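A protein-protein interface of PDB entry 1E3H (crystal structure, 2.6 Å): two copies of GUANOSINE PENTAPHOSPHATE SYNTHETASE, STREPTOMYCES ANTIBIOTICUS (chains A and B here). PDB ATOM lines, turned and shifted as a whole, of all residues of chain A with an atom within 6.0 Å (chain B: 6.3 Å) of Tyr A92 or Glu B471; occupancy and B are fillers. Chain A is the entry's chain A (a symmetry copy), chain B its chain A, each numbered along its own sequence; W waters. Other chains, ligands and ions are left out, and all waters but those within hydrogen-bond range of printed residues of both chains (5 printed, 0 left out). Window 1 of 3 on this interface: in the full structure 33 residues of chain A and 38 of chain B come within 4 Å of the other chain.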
ATOM      1  N   ARG A  90      18.713  17.021   1.988  1.00  0.00           N
ATOM      2  CA  ARG A  90      19.924  17.355   1.238  1.00  0.00           C
ATOM      3  C   ARG A  90      21.138  16.820   1.987  1.00  0.00           C
ATOM      4  O   ARG A  90      21.421  17.250   3.112  1.00  0.00           O
ATOM      5  CB  ARG A  90      20.056  18.869   1.059  1.00  0.00           C
ATOM      6  CG  ARG A  90      19.030  19.475   0.109  1.00  0.00           C
ATOM      7  CD  ARG A  90      19.388  19.230  -1.353  1.00  0.00           C
ATOM      8  NE  ARG A  90      18.490  19.948  -2.253  1.00  0.00           N
ATOM      9  CZ  ARG A  90      17.311  19.488  -2.666  1.00  0.00           C
ATOM     10  NH1 ARG A  90      16.884  18.298  -2.271  1.00  0.00           N
ATOM     11  NH2 ARG A  90      16.546  20.222  -3.466  1.00  0.00           N
ATOM     12  N   MET A  91      21.854  15.882   1.368  1.00  0.00           N
ATOM     13  CA  MET A  91      23.032  15.298   2.001  1.00  0.00           C
ATOM     14  C   MET A  91      24.069  16.341   2.395  1.00  0.00           C
ATOM     15  O   MET A  91      24.870  16.102   3.303  1.00  0.00           O
ATOM     16  CB  MET A  91      23.686  14.235   1.099  1.00  0.00           C
ATOM     17  CG  MET A  91      22.883  12.932   0.961  1.00  0.00           C
ATOM     18  SD  MET A  91      22.160  12.275   2.655  1.00  0.00           S
ATOM     19  CE  MET A  91      23.811  11.662   3.455  1.00  0.00           C
ATOM     20  N   TYR A  92      24.071  17.496   1.735  1.00  0.00           N
ATOM     21  CA  TYR A  92      25.049  18.507   2.106  1.00  0.00           C
ATOM     22  C   TYR A  92      24.756  19.047   3.505  1.00  0.00           C
ATOM     23  O   TYR A  92      25.604  19.681   4.129  1.00  0.00           O
ATOM     24  CB  TYR A  92      25.124  19.646   1.065  1.00  0.00           C
ATOM     25  CG  TYR A  92      23.859  20.444   0.809  1.00  0.00           C
ATOM     26  CD1 TYR A  92      23.241  21.186   1.826  1.00  0.00           C
ATOM     27  CD2 TYR A  92      23.310  20.512  -0.475  1.00  0.00           C
ATOM     28  CE1 TYR A  92      22.115  21.976   1.567  1.00  0.00           C
ATOM     29  CE2 TYR A  92      22.178  21.297  -0.745  1.00  0.00           C
ATOM     30  CZ  TYR A  92      21.591  22.025   0.276  1.00  0.00           C
ATOM     31  OH  TYR A  92      20.495  22.812  -0.007  1.00  0.00           O
ATOM     32  N   ALA A  93      23.558  18.767   4.009  1.00  0.00           N
ATOM     33  CA  ALA A  93      23.188  19.209   5.347  1.00  0.00           C
ATOM     34  C   ALA A  93      24.048  18.492   6.391  1.00  0.00           C
ATOM     35  O   ALA A  93      24.216  18.986   7.509  1.00  0.00           O
ATOM     36  CB  ALA A  93      21.715  18.930   5.607  1.00  0.00           C
ATOM     37  N   ALA A  94      24.581  17.329   6.021  1.00  0.00           N
ATOM     38  CA  ALA A  94      25.431  16.531   6.907  1.00  0.00           C
ATOM     39  C   ALA A  94      26.887  16.618   6.458  1.00  0.00           C
ATOM     40  O   ALA A  94      27.751  15.915   6.982  1.00  0.00           O
ATOM     41  CB  ALA A  94      24.985  15.075   6.898  1.00  0.00           C
ATOM     42  N   GLY A  95      27.146  17.467   5.464  1.00  0.00           N
ATOM     43  CA  GLY A  95      28.497  17.634   4.966  1.00  0.00           C
ATOM     44  C   GLY A  95      29.018  16.440   4.198  1.00  0.00           C
ATOM     45  O   GLY A  95      30.207  16.135   4.233  1.00  0.00           O
ATOM     46  N   LYS A  96      28.138  15.749   3.489  1.00  0.00           N
ATOM     47  CA  LYS A  96      28.595  14.603   2.729  1.00  0.00           C
ATOM     48  C   LYS A  96      27.994  14.502   1.334  1.00  0.00           C
ATOM     49  O   LYS A  96      26.889  14.963   1.076  1.00  0.00           O
ATOM     50  CB  LYS A  96      28.350  13.320   3.522  1.00  0.00           C
ATOM     51  CG  LYS A  96      26.925  13.088   3.893  1.00  0.00           C
ATOM     52  CD  LYS A  96      26.801  12.659   5.342  1.00  0.00           C
ATOM     53  CE  LYS A  96      27.302  11.261   5.598  1.00  0.00           C
ATOM     54  NZ  LYS A  96      27.030  10.894   7.022  1.00  0.00           N
ATOM     55  N   PRO A  98      26.319  12.524  -1.656  1.00  0.00           N
ATOM     56  CA  PRO A  98      25.481  11.319  -1.730  1.00  0.00           C
ATOM     57  C   PRO A  98      26.293  10.106  -2.176  1.00  0.00           C
ATOM     58  O   PRO A  98      27.075  10.181  -3.139  1.00  0.00           O
ATOM     59  CB  PRO A  98      24.410  11.701  -2.744  1.00  0.00           C
ATOM     60  CG  PRO A  98      24.281  13.186  -2.551  1.00  0.00           C
ATOM     61  CD  PRO A  98      25.726  13.631  -2.428  1.00  0.00           C
ATOM     62  N   GLU A 105      21.076  12.829  -4.477  1.00  0.00           N
ATOM     63  CA  GLU A 105      20.020  12.172  -3.721  1.00  0.00           C
ATOM     64  C   GLU A 105      18.772  11.997  -4.598  1.00  0.00           C
ATOM     65  O   GLU A 105      18.388  12.907  -5.337  1.00  0.00           O
ATOM     66  CB  GLU A 105      19.711  12.934  -2.409  1.00  0.00           C
ATOM     67  CG  GLU A 105      19.504  14.444  -2.482  1.00  0.00           C
ATOM     68  CD  GLU A 105      20.796  15.246  -2.600  1.00  0.00           C
ATOM     69  OE1 GLU A 105      21.398  15.620  -1.566  1.00  0.00           O
ATOM     70  OE2 GLU A 105      21.209  15.502  -3.743  1.00  0.00           O
ATOM     71  N   THR A 140      12.755  21.488   2.873  1.00  0.00           N
ATOM     72  CA  THR A 140      14.101  21.050   2.517  1.00  0.00           C
ATOM     73  C   THR A 140      15.002  21.081   3.760  1.00  0.00           C
ATOM     74  O   THR A 140      15.076  22.095   4.459  1.00  0.00           O
ATOM     75  CB  THR A 140      14.684  21.971   1.422  1.00  0.00           C
ATOM     76  OG1 THR A 140      13.777  22.015   0.315  1.00  0.00           O
ATOM     77  CG2 THR A 140      16.030  21.457   0.940  1.00  0.00           C
ATOM     78  N   ILE A 141      15.668  19.968   4.049  1.00  0.00           N
ATOM     79  CA  ILE A 141      16.553  19.905   5.204  1.00  0.00           C
ATOM     80  C   ILE A 141      17.906  20.377   4.694  1.00  0.00           C
ATOM     81  O   ILE A 141      18.600  19.642   3.994  1.00  0.00           O
ATOM     82  CB  ILE A 141      16.671  18.454   5.752  1.00  0.00           C
ATOM     83  CG1 ILE A 141      15.280  17.813   5.862  1.00  0.00           C
ATOM     84  CG2 ILE A 141      17.371  18.459   7.111  1.00  0.00           C
ATOM     85  CD1 ILE A 141      14.220  18.678   6.527  1.00  0.00           C
ATOM     86  N   MET A 142      18.275  21.605   5.044  1.00  0.00           N
ATOM     87  CA  MET A 142      19.525  22.199   4.573  1.00  0.00           C
ATOM     88  C   MET A 142      20.749  22.131   5.486  1.00  0.00           C
ATOM     89  O   MET A 142      21.875  22.145   5.010  1.00  0.00           O
ATOM     90  CB  MET A 142      19.252  23.641   4.168  1.00  0.00           C
ATOM     91  CG  MET A 142      18.176  23.731   3.110  1.00  0.00           C
ATOM     92  SD  MET A 142      17.936  25.500   2.379  1.00  0.00           S
ATOM     93  CE  MET A 142      19.527  26.283   3.058  1.00  0.00           C
ATOM     94  N   ALA A 143      20.542  22.070   6.792  1.00  0.00           N
ATOM     95  CA  ALA A 143      21.667  21.965   7.714  1.00  0.00           C
ATOM     96  C   ALA A 143      21.202  21.065   8.836  1.00  0.00           C
ATOM     97  O   ALA A 143      20.100  21.246   9.346  1.00  0.00           O
ATOM     98  CB  ALA A 143      22.043  23.326   8.255  1.00  0.00           C
ATOM     99  N   LEU A 409      20.165  11.169   6.142  1.00  0.00           N
ATOM    100  CA  LEU A 409      20.463  12.215   7.110  1.00  0.00           C
ATOM    101  C   LEU A 409      20.135  11.706   8.500  1.00  0.00           C
ATOM    102  O   LEU A 409      19.582  12.424   9.326  1.00  0.00           O
ATOM    103  CB  LEU A 409      19.630  13.462   6.828  1.00  0.00           C
ATOM    104  CG  LEU A 409      20.114  14.340   5.684  1.00  0.00           C
ATOM    105  CD1 LEU A 409      19.174  15.525   5.545  1.00  0.00           C
ATOM    106  CD2 LEU A 409      21.547  14.794   5.957  1.00  0.00           C
ATOM    107  N   ILE B 375      24.128  29.537   4.980  1.00  0.00           N
ATOM    108  CA  ILE B 375      23.567  28.349   5.616  1.00  0.00           C
ATOM    109  C   ILE B 375      24.503  27.841   6.710  1.00  0.00           C
ATOM    110  O   ILE B 375      25.715  27.799   6.531  1.00  0.00           O
ATOM    111  CB  ILE B 375      23.364  27.216   4.537  1.00  0.00           C
ATOM    112  CG1 ILE B 375      22.410  27.709   3.459  1.00  0.00           C
ATOM    113  CG2 ILE B 375      22.821  25.944   5.152  1.00  0.00           C
ATOM    114  CD1 ILE B 375      21.280  28.571   4.009  1.00  0.00           C
ATOM    115  N   ARG B 377      26.496  25.191   9.271  1.00  0.00           N
ATOM    116  CA  ARG B 377      27.146  23.886   9.147  1.00  0.00           C
ATOM    117  C   ARG B 377      27.776  23.467   7.812  1.00  0.00           C
ATOM    118  O   ARG B 377      28.863  22.880   7.801  1.00  0.00           O
ATOM    119  CB  ARG B 377      26.190  22.778   9.579  1.00  0.00           C
ATOM    120  CG  ARG B 377      25.627  22.921  10.976  1.00  0.00           C
ATOM    121  CD  ARG B 377      24.975  21.616  11.390  1.00  0.00           C
ATOM    122  NE  ARG B 377      25.981  20.573  11.549  1.00  0.00           N
ATOM    123  CZ  ARG B 377      26.760  20.447  12.621  1.00  0.00           C
ATOM    124  NH1 ARG B 377      26.641  21.298  13.635  1.00  0.00           N
ATOM    125  NH2 ARG B 377      27.672  19.483  12.673  1.00  0.00           N
ATOM    126  N   VAL B 378      27.115  23.735   6.692  1.00  0.00           N
ATOM    127  CA  VAL B 378      27.674  23.315   5.412  1.00  0.00           C
ATOM    128  C   VAL B 378      29.095  23.833   5.149  1.00  0.00           C
ATOM    129  O   VAL B 378      29.481  24.901   5.613  1.00  0.00           O
ATOM    130  CB  VAL B 378      26.754  23.714   4.246  1.00  0.00           C
ATOM    131  CG1 VAL B 378      25.375  23.095   4.461  1.00  0.00           C
ATOM    132  CG2 VAL B 378      26.669  25.237   4.129  1.00  0.00           C
ATOM    133  N   HIS B 379      29.866  23.056   4.399  1.00  0.00           N
ATOM    134  CA  HIS B 379      31.242  23.410   4.087  1.00  0.00           C
ATOM    135  C   HIS B 379      31.406  24.801   3.485  1.00  0.00           C
ATOM    136  O   HIS B 379      32.390  25.486   3.759  1.00  0.00           O
ATOM    137  CB  HIS B 379      31.838  22.343   3.169  1.00  0.00           C
ATOM    138  CG  HIS B 379      31.943  20.999   3.815  1.00  0.00           C
ATOM    139  ND1 HIS B 379      32.236  19.852   3.110  1.00  0.00           N
ATOM    140  CD2 HIS B 379      31.789  20.618   5.107  1.00  0.00           C
ATOM    141  CE1 HIS B 379      32.256  18.822   3.938  1.00  0.00           C
ATOM    142  NE2 HIS B 379      31.987  19.258   5.155  1.00  0.00           N
ATOM    143  N   GLN B 390      16.904  34.347  -7.488  1.00  0.00           N
ATOM    144  CA  GLN B 390      17.660  34.119  -6.267  1.00  0.00           C
ATOM    145  C   GLN B 390      18.211  32.697  -6.264  1.00  0.00           C
ATOM    146  O   GLN B 390      17.461  31.721  -6.380  1.00  0.00           O
ATOM    147  CB  GLN B 390      16.760  34.323  -5.051  1.00  0.00           C
ATOM    148  CG  GLN B 390      17.434  34.011  -3.729  1.00  0.00           C
ATOM    149  CD  GLN B 390      16.508  34.220  -2.542  1.00  0.00           C
ATOM    150  OE1 GLN B 390      15.513  33.512  -2.386  1.00  0.00           O
ATOM    151  NE2 GLN B 390      16.832  35.196  -1.702  1.00  0.00           N
ATOM    152  N   ILE B 391      19.523  32.582  -6.115  1.00  0.00           N
ATOM    153  CA  ILE B 391      20.162  31.280  -6.114  1.00  0.00           C
ATOM    154  C   ILE B 391      20.969  31.023  -4.860  1.00  0.00           C
ATOM    155  O   ILE B 391      21.802  31.834  -4.470  1.00  0.00           O
ATOM    156  CB  ILE B 391      21.134  31.131  -7.310  1.00  0.00           C
ATOM    157  CG1 ILE B 391      20.419  31.466  -8.631  1.00  0.00           C
ATOM    158  CG2 ILE B 391      21.729  29.729  -7.308  1.00  0.00           C
ATOM    159  CD1 ILE B 391      19.238  30.573  -8.957  1.00  0.00           C
ATOM    160  N   LEU B 392      20.721  29.884  -4.230  1.00  0.00           N
ATOM    161  CA  LEU B 392      21.473  29.490  -3.051  1.00  0.00           C
ATOM    162  C   LEU B 392      22.466  28.437  -3.523  1.00  0.00           C
ATOM    163  O   LEU B 392      22.081  27.446  -4.141  1.00  0.00           O
ATOM    164  CB  LEU B 392      20.563  28.868  -1.986  1.00  0.00           C
ATOM    165  CG  LEU B 392      21.316  28.286  -0.776  1.00  0.00           C
ATOM    166  CD1 LEU B 392      22.091  29.391  -0.068  1.00  0.00           C
ATOM    167  CD2 LEU B 392      20.344  27.632   0.184  1.00  0.00           C
ATOM    168  N   GLY B 393      23.743  28.660  -3.250  1.00  0.00           N
ATOM    169  CA  GLY B 393      24.753  27.693  -3.634  1.00  0.00           C
ATOM    170  C   GLY B 393      25.332  27.062  -2.381  1.00  0.00           C
ATOM    171  O   GLY B 393      25.589  27.764  -1.400  1.00  0.00           O
ATOM    172  N   VAL B 394      25.525  25.746  -2.394  1.00  0.00           N
ATOM    173  CA  VAL B 394      26.092  25.059  -1.241  1.00  0.00           C
ATOM    174  C   VAL B 394      27.210  24.122  -1.703  1.00  0.00           C
ATOM    175  O   VAL B 394      27.050  23.369  -2.668  1.00  0.00           O
ATOM    176  CB  VAL B 394      25.020  24.238  -0.468  1.00  0.00           C
ATOM    177  CG1 VAL B 394      25.673  23.502   0.697  1.00  0.00           C
ATOM    178  CG2 VAL B 394      23.924  25.156   0.055  1.00  0.00           C
ATOM    179  N   THR B 395      28.343  24.182  -1.009  1.00  0.00           N
ATOM    180  CA  THR B 395      29.500  23.356  -1.341  1.00  0.00           C
ATOM    181  C   THR B 395      29.731  22.269  -0.292  1.00  0.00           C
ATOM    182  O   THR B 395      29.546  22.498   0.904  1.00  0.00           O
ATOM    183  CB  THR B 395      30.778  24.216  -1.416  1.00  0.00           C
ATOM    184  OG1 THR B 395      30.549  25.324  -2.288  1.00  0.00           O
ATOM    185  CG2 THR B 395      31.953  23.402  -1.937  1.00  0.00           C
ATOM    186  N   THR B 396      30.134  21.091  -0.753  1.00  0.00           N
ATOM    187  CA  THR B 396      30.439  19.966   0.121  1.00  0.00           C
ATOM    188  C   THR B 396      31.794  19.420  -0.341  1.00  0.00           C
ATOM    189  O   THR B 396      32.023  19.241  -1.536  1.00  0.00           O
ATOM    190  CB  THR B 396      29.390  18.840   0.000  1.00  0.00           C
ATOM    191  OG1 THR B 396      28.096  19.338   0.357  1.00  0.00           O
ATOM    192  CG2 THR B 396      29.754  17.681   0.921  1.00  0.00           C
ATOM    193  N   ASN B 420      24.955  20.189  -9.271  1.00  0.00           N
ATOM    194  CA  ASN B 420      23.546  19.799  -9.348  1.00  0.00           C
ATOM    195  C   ASN B 420      22.724  21.071  -9.283  1.00  0.00           C
ATOM    196  O   ASN B 420      22.943  21.925  -8.429  1.00  0.00           O
ATOM    197  CB  ASN B 420      23.162  18.885  -8.188  1.00  0.00           C
ATOM    198  CG  ASN B 420      23.784  17.506  -8.298  1.00  0.00           C
ATOM    199  OD1 ASN B 420      23.884  16.782  -7.309  1.00  0.00           O
ATOM    200  ND2 ASN B 420      24.195  17.130  -9.506  1.00  0.00           N
ATOM    201  N   TYR B 421      21.777  21.195 -10.197  1.00  0.00           N
ATOM    202  CA  TYR B 421      20.931  22.370 -10.267  1.00  0.00           C
ATOM    203  C   TYR B 421      19.486  21.969  -9.996  1.00  0.00           C
ATOM    204  O   TYR B 421      18.925  21.150 -10.716  1.00  0.00           O
ATOM    205  CB  TYR B 421      21.084  23.000 -11.658  1.00  0.00           C
ATOM    206  CG  TYR B 421      20.080  24.066 -12.006  1.00  0.00           C
ATOM    207  CD1 TYR B 421      20.287  25.404 -11.662  1.00  0.00           C
ATOM    208  CD2 TYR B 421      18.908  23.729 -12.678  1.00  0.00           C
ATOM    209  CE1 TYR B 421      19.341  26.381 -11.986  1.00  0.00           C
ATOM    210  CE2 TYR B 421      17.960  24.684 -13.004  1.00  0.00           C
ATOM    211  CZ  TYR B 421      18.175  26.004 -12.658  1.00  0.00           C
ATOM    212  OH  TYR B 421      17.201  26.921 -12.989  1.00  0.00           O
ATOM    213  N   ASN B 422      18.900  22.539  -8.944  1.00  0.00           N
ATOM    214  CA  ASN B 422      17.516  22.261  -8.573  1.00  0.00           C
ATOM    215  C   ASN B 422      16.611  23.452  -8.831  1.00  0.00           C
ATOM    216  O   ASN B 422      16.902  24.577  -8.434  1.00  0.00           O
ATOM    217  CB  ASN B 422      17.419  21.883  -7.104  1.00  0.00           C
ATOM    218  CG  ASN B 422      18.154  20.610  -6.788  1.00  0.00           C
ATOM    219  OD1 ASN B 422      18.046  19.629  -7.521  1.00  0.00           O
ATOM    220  ND2 ASN B 422      18.898  20.606  -5.686  1.00  0.00           N
ATOM    221  N   PHE B 423      15.503  23.190  -9.500  1.00  0.00           N
ATOM    222  CA  PHE B 423      14.540  24.222  -9.825  1.00  0.00           C
ATOM    223  C   PHE B 423      13.170  23.762  -9.332  1.00  0.00           C
ATOM    224  O   PHE B 423      12.417  23.133 -10.064  1.00  0.00           O
ATOM    225  CB  PHE B 423      14.502  24.434 -11.337  1.00  0.00           C
ATOM    226  CG  PHE B 423      13.580  25.535 -11.765  1.00  0.00           C
ATOM    227  CD1 PHE B 423      14.023  26.855 -11.805  1.00  0.00           C
ATOM    228  CD2 PHE B 423      12.254  25.259 -12.101  1.00  0.00           C
ATOM    229  CE1 PHE B 423      13.160  27.886 -12.171  1.00  0.00           C
ATOM    230  CE2 PHE B 423      11.377  26.285 -12.469  1.00  0.00           C
ATOM    231  CZ  PHE B 423      11.832  27.601 -12.502  1.00  0.00           C
ATOM    232  N   PRO B 424      12.833  24.070  -8.077  1.00  0.00           N
ATOM    233  CA  PRO B 424      11.544  23.674  -7.503  1.00  0.00           C
ATOM    234  C   PRO B 424      10.386  24.535  -8.025  1.00  0.00           C
ATOM    235  O   PRO B 424      10.576  25.695  -8.384  1.00  0.00           O
ATOM    236  CB  PRO B 424      11.777  23.857  -6.007  1.00  0.00           C
ATOM    237  CG  PRO B 424      12.618  25.110  -5.977  1.00  0.00           C
ATOM    238  CD  PRO B 424      13.610  24.887  -7.126  1.00  0.00           C
ATOM    239  N   TYR B 426       7.962  26.060  -6.491  1.00  0.00           N
ATOM    240  CA  TYR B 426       7.745  27.276  -5.714  1.00  0.00           C
ATOM    241  C   TYR B 426       8.710  28.393  -6.102  1.00  0.00           C
ATOM    242  O   TYR B 426       8.558  29.543  -5.677  1.00  0.00           O
ATOM    243  CB  TYR B 426       7.820  26.982  -4.206  1.00  0.00           C
ATOM    244  CG  TYR B 426       9.161  26.533  -3.676  1.00  0.00           C
ATOM    245  CD1 TYR B 426      10.206  27.443  -3.490  1.00  0.00           C
ATOM    246  CD2 TYR B 426       9.376  25.194  -3.323  1.00  0.00           C
ATOM    247  CE1 TYR B 426      11.435  27.034  -2.959  1.00  0.00           C
ATOM    248  CE2 TYR B 426      10.596  24.772  -2.796  1.00  0.00           C
ATOM    249  CZ  TYR B 426      11.620  25.694  -2.616  1.00  0.00           C
ATOM    250  OH  TYR B 426      12.829  25.272  -2.106  1.00  0.00           O
ATOM    251  N   ARG B 467      31.323  18.750  -4.475  1.00  0.00           N
ATOM    252  CA  ARG B 467      29.952  18.744  -4.947  1.00  0.00           C
ATOM    253  C   ARG B 467      29.308  20.105  -4.722  1.00  0.00           C
ATOM    254  O   ARG B 467      29.163  20.556  -3.585  1.00  0.00           O
ATOM    255  CB  ARG B 467      29.125  17.685  -4.241  1.00  0.00           C
ATOM    256  CG  ARG B 467      27.795  17.475  -4.928  1.00  0.00           C
ATOM    257  CD  ARG B 467      26.804  16.869  -3.997  1.00  0.00           C
ATOM    258  NE  ARG B 467      25.524  16.679  -4.654  1.00  0.00           N
ATOM    259  CZ  ARG B 467      24.369  16.553  -4.009  1.00  0.00           C
ATOM    260  NH1 ARG B 467      24.329  16.601  -2.679  1.00  0.00           N
ATOM    261  NH2 ARG B 467      23.256  16.384  -4.704  1.00  0.00           N
ATOM    262  N   VAL B 469      25.948  22.443  -5.230  1.00  0.00           N
ATOM    263  CA  VAL B 469      24.505  22.386  -5.456  1.00  0.00           C
ATOM    264  C   VAL B 469      23.929  23.799  -5.538  1.00  0.00           C
ATOM    265  O   VAL B 469      24.227  24.642  -4.702  1.00  0.00           O
ATOM    266  CB  VAL B 469      23.782  21.623  -4.312  1.00  0.00           C
ATOM    267  CG1 VAL B 469      22.280  21.596  -4.566  1.00  0.00           C
ATOM    268  CG2 VAL B 469      24.325  20.205  -4.190  1.00  0.00           C
ATOM    269  N   SER B 470      23.117  24.058  -6.556  1.00  0.00           N
ATOM    270  CA  SER B 470      22.487  25.366  -6.722  1.00  0.00           C
ATOM    271  C   SER B 470      20.988  25.184  -6.562  1.00  0.00           C
ATOM    272  O   SER B 470      20.377  24.397  -7.286  1.00  0.00           O
ATOM    273  CB  SER B 470      22.765  25.943  -8.115  1.00  0.00           C
ATOM    274  OG  SER B 470      24.146  26.192  -8.312  1.00  0.00           O
ATOM    275  N   GLU B 471      20.392  25.902  -5.617  1.00  0.00           N
ATOM    276  CA  GLU B 471      18.956  25.800  -5.389  1.00  0.00           C
ATOM    277  C   GLU B 471      18.349  27.080  -5.937  1.00  0.00           C
ATOM    278  O   GLU B 471      18.610  28.156  -5.408  1.00  0.00           O
ATOM    279  CB  GLU B 471      18.641  25.707  -3.886  1.00  0.00           C
ATOM    280  CG  GLU B 471      19.502  24.733  -3.099  1.00  0.00           C
ATOM    281  CD  GLU B 471      19.049  23.282  -3.215  1.00  0.00           C
ATOM    282  OE1 GLU B 471      18.258  22.965  -4.139  1.00  0.00           O
ATOM    283  OE2 GLU B 471      19.502  22.456  -2.381  1.00  0.00           O
ATOM    284  N   ALA B 472      17.558  26.978  -6.999  1.00  0.00           N
ATOM    285  CA  ALA B 472      16.930  28.171  -7.557  1.00  0.00           C
ATOM    286  C   ALA B 472      15.697  28.467  -6.704  1.00  0.00           C
ATOM    287  O   ALA B 472      14.602  28.000  -7.013  1.00  0.00           O
ATOM    288  CB  ALA B 472      16.532  27.927  -9.013  1.00  0.00           C
ATOM    289  N   LEU B 473      15.879  29.233  -5.629  1.00  0.00           N
ATOM    290  CA  LEU B 473      14.781  29.548  -4.718  1.00  0.00           C
ATOM    291  C   LEU B 473      13.815  30.590  -5.260  1.00  0.00           C
ATOM    292  O   LEU B 473      12.668  30.668  -4.831  1.00  0.00           O
ATOM    293  CB  LEU B 473      15.337  30.018  -3.378  1.00  0.00           C
ATOM    294  CG  LEU B 473      16.274  29.042  -2.673  1.00  0.00           C
ATOM    295  CD1 LEU B 473      16.694  29.657  -1.355  1.00  0.00           C
ATOM    296  CD2 LEU B 473      15.585  27.683  -2.458  1.00  0.00           C
ATOM    297  N   GLY B 474      14.298  31.399  -6.195  1.00  0.00           N
ATOM    298  CA  GLY B 474      13.481  32.417  -6.822  1.00  0.00           C
ATOM    299  C   GLY B 474      13.902  32.455  -8.274  1.00  0.00           C
ATOM    300  O   GLY B 474      15.097  32.399  -8.567  1.00  0.00           O
HETATM  301  O   HOH W   1      13.409  22.485  -2.406  1.00  0.00           O
HETATM  302  O   HOH W   2      12.000  24.112   0.589  1.00  0.00           O
HETATM  303  O   HOH W   3      26.670  18.982   9.138  1.00  0.00           O
HETATM  304  O   HOH W   4      28.264  20.675   3.327  1.00  0.00           O
HETATM  305  O   HOH W   5      26.661  17.130  -0.811  1.00  0.00           O
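Water W2 lies within hydrogen-bond range of the side-chain hydroxyl of Thr A140 (2.8 Å) and the side-chain hydroxyl of Tyr B426 (3.0 Å). Water W1 lies within hydrogen-bond range of the side-chain hydroxyl (OG1) of Thr A140 and the side-chain hydroxyl (OH) of Tyr B426. Water W5 lies within hydrogen-bond range of the side-chain hydroxyl (OG1) of Thr B396, the backbone carbonyl oxygen (O) of Lys A96 and the guanidinium group (NH1) of Arg B467. Water W3 lies within hydrogen-bond range of the backbone carbonyl oxygen of Ala A93 and the guanidinium group of Arg B377. Water W4 lies within hydrogen-bond range of O of Tyr A92, N of His B379, OG1 of Thr B396 and O of Thr B395.
Printed residues of chain B that touch a printed residue of chain A: Ile B375, Val B378, His B379, Leu B392, Val B394, Thr B396, Asn B422, Arg B467, Val B469 and Glu B471.
Of the printed residues of chain B, Arg A90 touches Asn B422 (3.3 Å) and Glu B471 (2.7 Å). Of chain B, only Val B378 (3.4 Å), Val B394 (3.5 Å), Thr B396 (3.1 Å), Val B469 (3.8 Å) and Glu B471 (2.6 Å) come within 4 Å of Tyr A92. Printed residues of chain B within 4 Å of Glu A105: Arg B467 (2.4 Å). Printed residues of chain B within 4 Å of Met A142: Ile B375 (3.0 Å), Val B378 (3.7 Å) and Leu B392 (3.3 Å). Printed residues of chain A within 4 Å of Val B378: Tyr A92 and Met A142. Ile B391 touches none of the printed residues of chain A. Of the printed residues of chain A, Glu B471 touches Arg A90 (2.7 Å) and Tyr A92 (2.6 Å). Ala B472 touches none of the printed residues of chain A. The nearest residue of chain B that does not touch Tyr A92 is Arg B467 (4.5 Å). The nearest printed residue of chain B that does not touch Glu A105 is Asn B420 (4.6 Å).
The side-chain amide nitrogen (ND2) of Asn B422 is in hydrogen-bond range of the side-chain carboxylate (OE1) of Glu B471, 2.9 Å away. The backbone NH of Met A91 lies within hydrogen-bond range of the side-chain carboxylate of Glu A105, at 3.0 Å. The backbone carbonyl oxygen of Leu B392 is in hydrogen-bond range of the backbone NH of Glu B471, 2.7 Å away. The backbone NH (N) of Thr B396 lies within hydrogen-bond range of the backbone carbonyl oxygen (O) of Arg B467. The side-chain amide oxygen (OD1) of Asn B420 lies within hydrogen-bond range of the guanidinium group (NH2) of Arg B467 (2.7 Å). The backbone NH (N) of Asn B422 is in hydrogen-bond range of the backbone carbonyl oxygen (O) of Ser B470, at 2.9 Å.
No position is printed for both chains. Of the 15 pairs that touch across the chains among the printed residues, none has its exchanged pair printed and touching as well.
Among the printed residues, pairs that only touch across the chains: Tyr A92 with Val B378, Tyr A92 with Val B394, Tyr A92 with Thr B396, Tyr A92 with Val B469, Gly A95 with His B379, Gly A95 with Thr B396, Lys A96 with Thr B396, Pro A98 with Arg B467, Met A142 with Ile B375, Met A142 with Val B378 and Met A142 with Leu B392.
ND2 of Asn B422 lies close to NH2 of Arg A90, 3.3 Å away. OH of Tyr A92 lies within hydrogen-bond range of OE2 of Glu B471, at 2.6 Å. The guanidinium group (NH2) of Arg B467 is in salt-bridge range of the side-chain carboxylate (OE2) of Glu A105 (2.4 Å). The side-chain carboxylate of Glu B471 is in salt-bridge range of the guanidinium group of Arg A90 (2.7 Å).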
